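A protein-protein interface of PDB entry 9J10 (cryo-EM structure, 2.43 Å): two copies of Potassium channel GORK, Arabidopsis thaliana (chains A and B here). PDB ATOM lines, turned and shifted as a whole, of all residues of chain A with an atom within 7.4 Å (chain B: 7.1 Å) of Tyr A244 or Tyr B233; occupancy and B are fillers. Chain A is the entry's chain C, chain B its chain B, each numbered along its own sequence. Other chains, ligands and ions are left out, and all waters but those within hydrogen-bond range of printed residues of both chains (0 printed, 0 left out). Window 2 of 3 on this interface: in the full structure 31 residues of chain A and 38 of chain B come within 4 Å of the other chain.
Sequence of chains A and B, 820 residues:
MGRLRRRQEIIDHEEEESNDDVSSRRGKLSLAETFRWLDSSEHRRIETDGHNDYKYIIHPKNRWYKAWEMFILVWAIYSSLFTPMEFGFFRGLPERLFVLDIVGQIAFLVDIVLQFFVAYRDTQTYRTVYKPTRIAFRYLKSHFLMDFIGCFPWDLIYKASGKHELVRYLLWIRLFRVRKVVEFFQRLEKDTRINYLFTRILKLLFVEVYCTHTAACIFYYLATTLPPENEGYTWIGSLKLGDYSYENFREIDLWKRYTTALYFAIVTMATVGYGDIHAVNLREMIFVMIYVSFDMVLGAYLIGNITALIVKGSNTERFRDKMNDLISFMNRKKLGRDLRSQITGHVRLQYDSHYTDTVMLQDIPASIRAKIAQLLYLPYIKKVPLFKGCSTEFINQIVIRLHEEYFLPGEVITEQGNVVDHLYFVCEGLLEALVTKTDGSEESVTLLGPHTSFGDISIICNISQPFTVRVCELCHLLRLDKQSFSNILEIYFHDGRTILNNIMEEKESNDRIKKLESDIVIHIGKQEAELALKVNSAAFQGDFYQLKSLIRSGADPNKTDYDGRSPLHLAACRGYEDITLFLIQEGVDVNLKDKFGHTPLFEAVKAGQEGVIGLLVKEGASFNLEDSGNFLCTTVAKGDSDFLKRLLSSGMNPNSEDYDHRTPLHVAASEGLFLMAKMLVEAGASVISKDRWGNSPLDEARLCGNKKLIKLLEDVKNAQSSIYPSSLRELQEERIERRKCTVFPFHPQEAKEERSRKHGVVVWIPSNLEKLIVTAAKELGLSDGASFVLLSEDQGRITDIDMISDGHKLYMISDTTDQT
The side-chain carboxylate (OD1) of Asp A243 lies close to the backbone carbonyl oxygen (O) of Gly B232 (3.3 Å). The side-chain hydroxyl of Tyr B233 is in hydrogen-bond range of the side-chain amino group of Lys A256 (3.3 Å).
The side-chain carboxylate (OE1) of Glu B284 sits at hydrogen-bond distance from the backbone NH (N) of Val B280, at 3.2 Å. O of Tyr B233 lies close to OD1 of Asn B281 (3.1 Å).
Among the printed residues, pairs that only touch across the chains: Leu A241 with Met B285 (3.8 Å), Gly A242 with Gly B232 (3.96 Å), Gly A242 with Val B280 (3.9 Å), Asp A243 with Tyr B233 (3.7 Å), Tyr A244 with Tyr B233 (3.7 Å) and Lys A256 with Leu B282 (3.8 Å).
Of the printed residues of chain B, Leu A241 touches Met B285 (3.8 Å). Printed residues of chain B within 4 Å of Gly A242: Gly B232 and Val B280. Of the printed residues of chain B, Asp A243 touches Gly B232 (3.3 Å) and Tyr B233 (3.7 Å). Of chain B, only Tyr B233 (3.7 Å) comes within 4 Å of Tyr A244. Of the printed residues of chain B, Lys A256 touches Tyr B233 (3.3 Å) and Leu B282 (3.8 Å). Printed residues of chain A within 4 Å of Gly B232: Gly A242 (3.96 Å) and Asp A243 (3.3 Å). Of chain A, only Asp A243, Tyr A244 and Lys A256 come within 4 Å of Tyr B233. Printed residues of chain A within 4 Å of Leu B282: Lys A256. The nearest residue of chain B that does not touch Tyr A244 is Gly B232 (5.9 Å). The nearest residue of chain A that does not touch Tyr B233 is Leu A241 (4.03 Å). The nearest printed residue of chain B that does not touch Leu A241 is Tyr B233 (4.03 Å).
Of the 16 printed residues of chain B, 5 touch a printed residue of chain A. Of the 12 printed residues of chain A, 5 touch a printed residue of chain B. Among the printed residues, 8 pairs touch across the chains.
No position is printed for both chains.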
ATOM      1  N   LEU A 239     -13.076 -21.903  16.018  1.00  0.00           N
ATOM      2  CA  LEU A 239     -13.407 -20.684  16.736  1.00  0.00           C
ATOM      3  C   LEU A 239     -12.919 -20.756  18.176  1.00  0.00           C
ATOM      4  O   LEU A 239     -12.921 -21.821  18.794  1.00  0.00           O
ATOM      5  CB  LEU A 239     -14.917 -20.458  16.698  1.00  0.00           C
ATOM      6  CG  LEU A 239     -15.546 -19.258  17.398  1.00  0.00           C
ATOM      7  CD1 LEU A 239     -15.076 -17.980  16.756  1.00  0.00           C
ATOM      8  CD2 LEU A 239     -17.044 -19.365  17.334  1.00  0.00           C
ATOM      9  N   LYS A 240     -12.501 -19.613  18.709  1.00  0.00           N
ATOM     10  CA  LYS A 240     -12.039 -19.513  20.086  1.00  0.00           C
ATOM     11  C   LYS A 240     -12.404 -18.129  20.599  1.00  0.00           C
ATOM     12  O   LYS A 240     -12.025 -17.126  19.993  1.00  0.00           O
ATOM     13  CB  LYS A 240     -10.530 -19.755  20.162  1.00  0.00           C
ATOM     14  CG  LYS A 240      -9.846 -19.185  21.373  1.00  0.00           C
ATOM     15  CD  LYS A 240      -9.588 -20.264  22.400  1.00  0.00           C
ATOM     16  CE  LYS A 240      -8.783 -19.733  23.571  1.00  0.00           C
ATOM     17  NZ  LYS A 240      -8.527 -20.791  24.581  1.00  0.00           N
ATOM     18  N   LEU A 241     -13.154 -18.068  21.695  1.00  0.00           N
ATOM     19  CA  LEU A 241     -13.663 -16.807  22.230  1.00  0.00           C
ATOM     20  C   LEU A 241     -13.331 -16.737  23.711  1.00  0.00           C
ATOM     21  O   LEU A 241     -13.842 -17.535  24.500  1.00  0.00           O
ATOM     22  CB  LEU A 241     -15.170 -16.685  22.021  1.00  0.00           C
ATOM     23  CG  LEU A 241     -15.675 -16.331  20.627  1.00  0.00           C
ATOM     24  CD1 LEU A 241     -17.177 -16.416  20.593  1.00  0.00           C
ATOM     25  CD2 LEU A 241     -15.217 -14.952  20.228  1.00  0.00           C
ATOM     26  N   GLY A 242     -12.497 -15.781  24.091  1.00  0.00           N
ATOM     27  CA  GLY A 242     -12.085 -15.695  25.481  1.00  0.00           C
ATOM     28  C   GLY A 242     -11.118 -16.809  25.791  1.00  0.00           C
ATOM     29  O   GLY A 242     -10.102 -16.980  25.114  1.00  0.00           O
ATOM     30  N   ASP A 243     -11.436 -17.600  26.811  1.00  0.00           N
ATOM     31  CA  ASP A 243     -10.669 -18.798  27.115  1.00  0.00           C
ATOM     32  C   ASP A 243     -11.468 -20.073  26.873  1.00  0.00           C
ATOM     33  O   ASP A 243     -11.170 -21.110  27.468  1.00  0.00           O
ATOM     34  CB  ASP A 243     -10.142 -18.748  28.550  1.00  0.00           C
ATOM     35  CG  ASP A 243     -11.240 -18.631  29.587  1.00  0.00           C
ATOM     36  OD1 ASP A 243     -12.411 -18.410  29.231  1.00  0.00           O
ATOM     37  OD2 ASP A 243     -10.923 -18.760  30.783  1.00  0.00           O
ATOM     38  N   TYR A 244     -12.470 -20.017  26.005  1.00  0.00           N
ATOM     39  CA  TYR A 244     -13.314 -21.156  25.687  1.00  0.00           C
ATOM     40  C   TYR A 244     -13.072 -21.585  24.247  1.00  0.00           C
ATOM     41  O   TYR A 244     -12.979 -20.746  23.349  1.00  0.00           O
ATOM     42  CB  TYR A 244     -14.789 -20.813  25.888  1.00  0.00           C
ATOM     43  CG  TYR A 244     -15.728 -21.934  25.544  1.00  0.00           C
ATOM     44  CD1 TYR A 244     -15.853 -23.031  26.377  1.00  0.00           C
ATOM     45  CD2 TYR A 244     -16.493 -21.898  24.389  1.00  0.00           C
ATOM     46  CE1 TYR A 244     -16.706 -24.060  26.070  1.00  0.00           C
ATOM     47  CE2 TYR A 244     -17.347 -22.926  24.073  1.00  0.00           C
ATOM     48  CZ  TYR A 244     -17.449 -24.002  24.919  1.00  0.00           C
ATOM     49  OH  TYR A 244     -18.301 -25.030  24.615  1.00  0.00           O
ATOM     50  N   SER A 245     -12.990 -22.891  24.027  1.00  0.00           N
ATOM     51  CA  SER A 245     -12.713 -23.442  22.711  1.00  0.00           C
ATOM     52  C   SER A 245     -13.916 -24.216  22.201  1.00  0.00           C
ATOM     53  O   SER A 245     -14.542 -24.973  22.944  1.00  0.00           O
ATOM     54  CB  SER A 245     -11.494 -24.353  22.742  1.00  0.00           C
ATOM     55  OG  SER A 245     -11.272 -24.926  21.473  1.00  0.00           O
ATOM     56  N   TYR A 246     -14.223 -24.035  20.919  1.00  0.00           N
ATOM     57  CA  TYR A 246     -15.385 -24.639  20.286  1.00  0.00           C
ATOM     58  C   TYR A 246     -15.050 -25.942  19.575  1.00  0.00           C
ATOM     59  O   TYR A 246     -15.732 -26.311  18.620  1.00  0.00           O
ATOM     60  CB  TYR A 246     -16.010 -23.666  19.291  1.00  0.00           C
ATOM     61  CG  TYR A 246     -16.996 -22.685  19.868  1.00  0.00           C
ATOM     62  CD1 TYR A 246     -18.356 -22.898  19.747  1.00  0.00           C
ATOM     63  CD2 TYR A 246     -16.570 -21.527  20.496  1.00  0.00           C
ATOM     64  CE1 TYR A 246     -19.265 -22.005  20.257  1.00  0.00           C
ATOM     65  CE2 TYR A 246     -17.473 -20.625  21.007  1.00  0.00           C
ATOM     66  CZ  TYR A 246     -18.819 -20.872  20.884  1.00  0.00           C
ATOM     67  OH  TYR A 246     -19.729 -19.980  21.391  1.00  0.00           O
ATOM     68  N   GLU A 247     -14.015 -26.647  20.010  1.00  0.00           N
ATOM     69  CA  GLU A 247     -13.662 -27.893  19.350  1.00  0.00           C
ATOM     70  C   GLU A 247     -14.606 -29.003  19.788  1.00  0.00           C
ATOM     71  O   GLU A 247     -15.244 -28.918  20.838  1.00  0.00           O
ATOM     72  CB  GLU A 247     -12.217 -28.280  19.653  1.00  0.00           C
ATOM     73  CG  GLU A 247     -11.965 -28.669  21.091  1.00  0.00           C
ATOM     74  CD  GLU A 247     -10.541 -28.404  21.527  1.00  0.00           C
ATOM     75  OE1 GLU A 247      -9.723 -27.994  20.677  1.00  0.00           O
ATOM     76  OE2 GLU A 247     -10.237 -28.606  22.720  1.00  0.00           O
ATOM     77  N   ILE A 252     -21.585 -29.985  21.785  1.00  0.00           N
ATOM     78  CA  ILE A 252     -22.053 -28.798  22.486  1.00  0.00           C
ATOM     79  C   ILE A 252     -23.574 -28.776  22.407  1.00  0.00           C
ATOM     80  O   ILE A 252     -24.157 -29.207  21.408  1.00  0.00           O
ATOM     81  CB  ILE A 252     -21.410 -27.543  21.859  1.00  0.00           C
ATOM     82  CG1 ILE A 252     -19.891 -27.676  21.874  1.00  0.00           C
ATOM     83  CG2 ILE A 252     -21.788 -26.278  22.591  1.00  0.00           C
ATOM     84  CD1 ILE A 252     -19.177 -26.579  21.145  1.00  0.00           C
ATOM     85  N   ASP A 253     -24.233 -28.289  23.460  1.00  0.00           N
ATOM     86  CA  ASP A 253     -25.688 -28.312  23.488  1.00  0.00           C
ATOM     87  C   ASP A 253     -26.267 -27.291  22.512  1.00  0.00           C
ATOM     88  O   ASP A 253     -25.567 -26.424  21.990  1.00  0.00           O
ATOM     89  CB  ASP A 253     -26.211 -28.049  24.895  1.00  0.00           C
ATOM     90  CG  ASP A 253     -25.838 -26.692  25.403  1.00  0.00           C
ATOM     91  OD1 ASP A 253     -24.627 -26.427  25.524  1.00  0.00           O
ATOM     92  OD2 ASP A 253     -26.747 -25.889  25.691  1.00  0.00           O
ATOM     93  N   LYS A 256     -26.495 -23.057  22.659  1.00  0.00           N
ATOM     94  CA  LYS A 256     -25.235 -22.340  22.514  1.00  0.00           C
ATOM     95  C   LYS A 256     -24.837 -22.213  21.047  1.00  0.00           C
ATOM     96  O   LYS A 256     -24.454 -21.127  20.591  1.00  0.00           O
ATOM     97  CB  LYS A 256     -24.155 -23.057  23.314  1.00  0.00           C
ATOM     98  CG  LYS A 256     -22.845 -22.331  23.402  1.00  0.00           C
ATOM     99  CD  LYS A 256     -22.149 -22.676  24.693  1.00  0.00           C
ATOM    100  CE  LYS A 256     -20.878 -21.882  24.865  1.00  0.00           C
ATOM    101  NZ  LYS A 256     -20.308 -22.054  26.222  1.00  0.00           N
ATOM    102  N   LEU B 226     -20.578 -12.430  36.877  1.00  0.00           N
ATOM    103  CA  LEU B 226     -19.779 -13.634  36.998  1.00  0.00           C
ATOM    104  C   LEU B 226     -18.803 -13.492  38.161  1.00  0.00           C
ATOM    105  O   LEU B 226     -18.446 -12.373  38.528  1.00  0.00           O
ATOM    106  CB  LEU B 226     -19.014 -13.904  35.700  1.00  0.00           C
ATOM    107  CG  LEU B 226     -19.888 -14.292  34.512  1.00  0.00           C
ATOM    108  CD1 LEU B 226     -19.051 -14.473  33.287  1.00  0.00           C
ATOM    109  CD2 LEU B 226     -20.630 -15.563  34.807  1.00  0.00           C
ATOM    110  N   GLU B 229     -13.293 -15.493  39.626  1.00  0.00           N
ATOM    111  CA  GLU B 229     -12.470 -16.601  39.172  1.00  0.00           C
ATOM    112  C   GLU B 229     -12.774 -16.998  37.736  1.00  0.00           C
ATOM    113  O   GLU B 229     -11.942 -17.644  37.098  1.00  0.00           O
ATOM    114  CB  GLU B 229     -12.655 -17.804  40.096  1.00  0.00           C
ATOM    115  CG  GLU B 229     -12.123 -17.598  41.505  1.00  0.00           C
ATOM    116  CD  GLU B 229     -13.131 -16.941  42.431  1.00  0.00           C
ATOM    117  OE1 GLU B 229     -14.278 -16.713  42.001  1.00  0.00           O
ATOM    118  OE2 GLU B 229     -12.770 -16.652  43.591  1.00  0.00           O
ATOM    119  N   ASN B 230     -13.936 -16.614  37.212  1.00  0.00           N
ATOM    120  CA  ASN B 230     -14.268 -16.780  35.803  1.00  0.00           C
ATOM    121  C   ASN B 230     -14.072 -15.490  35.028  1.00  0.00           C
ATOM    122  O   ASN B 230     -14.835 -15.192  34.106  1.00  0.00           O
ATOM    123  CB  ASN B 230     -15.699 -17.282  35.650  1.00  0.00           C
ATOM    124  CG  ASN B 230     -15.957 -18.530  36.443  1.00  0.00           C
ATOM    125  OD1 ASN B 230     -15.029 -19.247  36.802  1.00  0.00           O
ATOM    126  ND2 ASN B 230     -17.219 -18.799  36.731  1.00  0.00           N
ATOM    127  N   GLU B 231     -13.056 -14.719  35.402  1.00  0.00           N
ATOM    128  CA  GLU B 231     -12.822 -13.406  34.823  1.00  0.00           C
ATOM    129  C   GLU B 231     -12.396 -13.488  33.363  1.00  0.00           C
ATOM    130  O   GLU B 231     -12.707 -12.588  32.579  1.00  0.00           O
ATOM    131  CB  GLU B 231     -11.766 -12.690  35.655  1.00  0.00           C
ATOM    132  CG  GLU B 231     -11.592 -11.247  35.350  1.00  0.00           C
ATOM    133  CD  GLU B 231     -10.232 -10.757  35.749  1.00  0.00           C
ATOM    134  OE1 GLU B 231      -9.316 -11.586  35.899  1.00  0.00           O
ATOM    135  OE2 GLU B 231     -10.074  -9.535  35.893  1.00  0.00           O
ATOM    136  N   GLY B 232     -11.723 -14.567  32.972  1.00  0.00           N
ATOM    137  CA  GLY B 232     -11.237 -14.697  31.612  1.00  0.00           C
ATOM    138  C   GLY B 232     -12.293 -15.043  30.586  1.00  0.00           C
ATOM    139  O   GLY B 232     -11.959 -15.174  29.407  1.00  0.00           O
ATOM    140  N   TYR B 233     -13.544 -15.195  30.998  1.00  0.00           N
ATOM    141  CA  TYR B 233     -14.654 -15.476  30.100  1.00  0.00           C
ATOM    142  C   TYR B 233     -15.586 -14.268  30.009  1.00  0.00           C
ATOM    143  O   TYR B 233     -16.800 -14.400  29.883  1.00  0.00           O
ATOM    144  CB  TYR B 233     -15.395 -16.729  30.562  1.00  0.00           C
ATOM    145  CG  TYR B 233     -16.279 -17.386  29.529  1.00  0.00           C
ATOM    146  CD1 TYR B 233     -15.944 -17.369  28.186  1.00  0.00           C
ATOM    147  CD2 TYR B 233     -17.450 -18.026  29.901  1.00  0.00           C
ATOM    148  CE1 TYR B 233     -16.754 -17.966  27.246  1.00  0.00           C
ATOM    149  CE2 TYR B 233     -18.262 -18.625  28.966  1.00  0.00           C
ATOM    150  CZ  TYR B 233     -17.908 -18.590  27.643  1.00  0.00           C
ATOM    151  OH  TYR B 233     -18.712 -19.185  26.705  1.00  0.00           O
ATOM    152  N   THR B 234     -15.024 -13.064  30.086  1.00  0.00           N
ATOM    153  CA  THR B 234     -15.773 -11.827  29.925  1.00  0.00           C
ATOM    154  C   THR B 234     -15.113 -10.972  28.857  1.00  0.00           C
ATOM    155  O   THR B 234     -14.010 -11.260  28.396  1.00  0.00           O
ATOM    156  CB  THR B 234     -15.872 -11.035  31.234  1.00  0.00           C
ATOM    157  OG1 THR B 234     -14.562 -10.795  31.749  1.00  0.00           O
ATOM    158  CG2 THR B 234     -16.671 -11.787  32.258  1.00  0.00           C
ATOM    159  N   TRP B 235     -15.804  -9.902  28.463  1.00  0.00           N
ATOM    160  CA  TRP B 235     -15.290  -9.053  27.398  1.00  0.00           C
ATOM    161  C   TRP B 235     -14.163  -8.161  27.883  1.00  0.00           C
ATOM    162  O   TRP B 235     -13.280  -7.809  27.101  1.00  0.00           O
ATOM    163  CB  TRP B 235     -16.415  -8.212  26.791  1.00  0.00           C
ATOM    164  CG  TRP B 235     -16.988  -7.131  27.673  1.00  0.00           C
ATOM    165  CD1 TRP B 235     -18.081  -7.231  28.470  1.00  0.00           C
ATOM    166  CD2 TRP B 235     -16.520  -5.783  27.809  1.00  0.00           C
ATOM    167  NE1 TRP B 235     -18.315  -6.046  29.108  1.00  0.00           N
ATOM    168  CE2 TRP B 235     -17.369  -5.140  28.720  1.00  0.00           C
ATOM    169  CE3 TRP B 235     -15.458  -5.066  27.259  1.00  0.00           C
ATOM    170  CZ2 TRP B 235     -17.192  -3.814  29.093  1.00  0.00           C
ATOM    171  CZ3 TRP B 235     -15.283  -3.755  27.630  1.00  0.00           C
ATOM    172  CH2 TRP B 235     -16.145  -3.139  28.536  1.00  0.00           C
ATOM    173  N   ILE B 236     -14.167  -7.790  29.157  1.00  0.00           N
ATOM    174  CA  ILE B 236     -13.140  -6.893  29.663  1.00  0.00           C
ATOM    175  C   ILE B 236     -12.032  -7.659  30.382  1.00  0.00           C
ATOM    176  O   ILE B 236     -10.870  -7.254  30.329  1.00  0.00           O
ATOM    177  CB  ILE B 236     -13.786  -5.810  30.555  1.00  0.00           C
ATOM    178  CG1 ILE B 236     -12.765  -4.769  31.014  1.00  0.00           C
ATOM    179  CG2 ILE B 236     -14.527  -6.412  31.726  1.00  0.00           C
ATOM    180  CD1 ILE B 236     -13.380  -3.555  31.636  1.00  0.00           C
ATOM    181  N   GLY B 237     -12.343  -8.809  30.980  1.00  0.00           N
ATOM    182  CA  GLY B 237     -11.331  -9.569  31.686  1.00  0.00           C
ATOM    183  C   GLY B 237     -10.351 -10.286  30.785  1.00  0.00           C
ATOM    184  O   GLY B 237      -9.318 -10.755  31.268  1.00  0.00           O
ATOM    185  N   SER B 238     -10.641 -10.370  29.491  1.00  0.00           N
ATOM    186  CA  SER B 238      -9.740 -10.989  28.531  1.00  0.00           C
ATOM    187  C   SER B 238      -9.208  -9.999  27.506  1.00  0.00           C
ATOM    188  O   SER B 238      -8.642 -10.418  26.495  1.00  0.00           O
ATOM    189  CB  SER B 238     -10.444 -12.143  27.822  1.00  0.00           C
ATOM    190  OG  SER B 238     -11.593 -11.687  27.143  1.00  0.00           O
ATOM    191  N   VAL B 280     -17.960 -12.164  24.251  1.00  0.00           N
ATOM    192  CA  VAL B 280     -17.525 -13.555  24.321  1.00  0.00           C
ATOM    193  C   VAL B 280     -18.526 -14.466  25.013  1.00  0.00           C
ATOM    194  O   VAL B 280     -18.426 -15.694  24.874  1.00  0.00           O
ATOM    195  CB  VAL B 280     -16.145 -13.678  25.010  1.00  0.00           C
ATOM    196  CG1 VAL B 280     -15.077 -12.872  24.293  1.00  0.00           C
ATOM    197  CG2 VAL B 280     -16.235 -13.279  26.442  1.00  0.00           C
ATOM    198  N   ASN B 281     -19.499 -13.949  25.748  1.00  0.00           N
ATOM    199  CA  ASN B 281     -20.450 -14.743  26.510  1.00  0.00           C
ATOM    200  C   ASN B 281     -21.720 -14.975  25.706  1.00  0.00           C
ATOM    201  O   ASN B 281     -21.835 -14.568  24.556  1.00  0.00           O
ATOM    202  CB  ASN B 281     -20.812 -14.035  27.809  1.00  0.00           C
ATOM    203  CG  ASN B 281     -20.035 -14.540  28.968  1.00  0.00           C
ATOM    204  OD1 ASN B 281     -19.497 -15.637  28.930  1.00  0.00           O
ATOM    205  ND2 ASN B 281     -19.967 -13.746  30.020  1.00  0.00           N
ATOM    206  N   LEU B 282     -22.698 -15.620  26.336  1.00  0.00           N
ATOM    207  CA  LEU B 282     -24.012 -15.715  25.710  1.00  0.00           C
ATOM    208  C   LEU B 282     -24.905 -14.542  26.083  1.00  0.00           C
ATOM    209  O   LEU B 282     -25.679 -14.068  25.245  1.00  0.00           O
ATOM    210  CB  LEU B 282     -24.693 -17.030  26.072  1.00  0.00           C
ATOM    211  CG  LEU B 282     -24.464 -18.222  25.148  1.00  0.00           C
ATOM    212  CD1 LEU B 282     -23.071 -18.794  25.258  1.00  0.00           C
ATOM    213  CD2 LEU B 282     -25.493 -19.277  25.458  1.00  0.00           C
ATOM    214  N   GLU B 284     -23.870 -11.510  26.751  1.00  0.00           N
ATOM    215  CA  GLU B 284     -23.370 -10.354  26.024  1.00  0.00           C
ATOM    216  C   GLU B 284     -23.785 -10.409  24.562  1.00  0.00           C
ATOM    217  O   GLU B 284     -24.080  -9.370  23.960  1.00  0.00           O
ATOM    218  CB  GLU B 284     -21.855 -10.283  26.151  1.00  0.00           C
ATOM    219  CG  GLU B 284     -21.385 -10.057  27.564  1.00  0.00           C
ATOM    220  CD  GLU B 284     -19.934 -10.426  27.770  1.00  0.00           C
ATOM    221  OE1 GLU B 284     -19.268 -10.809  26.793  1.00  0.00           O
ATOM    222  OE2 GLU B 284     -19.454 -10.324  28.916  1.00  0.00           O
ATOM    223  N   MET B 285     -23.850 -11.615  23.992  1.00  0.00           N
ATOM    224  CA  MET B 285     -24.316 -11.782  22.620  1.00  0.00           C
ATOM    225  C   MET B 285     -25.780 -11.393  22.480  1.00  0.00           C
ATOM    226  O   MET B 285     -26.165 -10.739  21.504  1.00  0.00           O
ATOM    227  CB  MET B 285     -24.118 -13.227  22.167  1.00  0.00           C
ATOM    228  CG  MET B 285     -22.748 -13.559  21.619  1.00  0.00           C
ATOM    229  SD  MET B 285     -22.601 -15.325  21.313  1.00  0.00           S
ATOM    230  CE  MET B 285     -20.833 -15.528  21.237  1.00  0.00           C
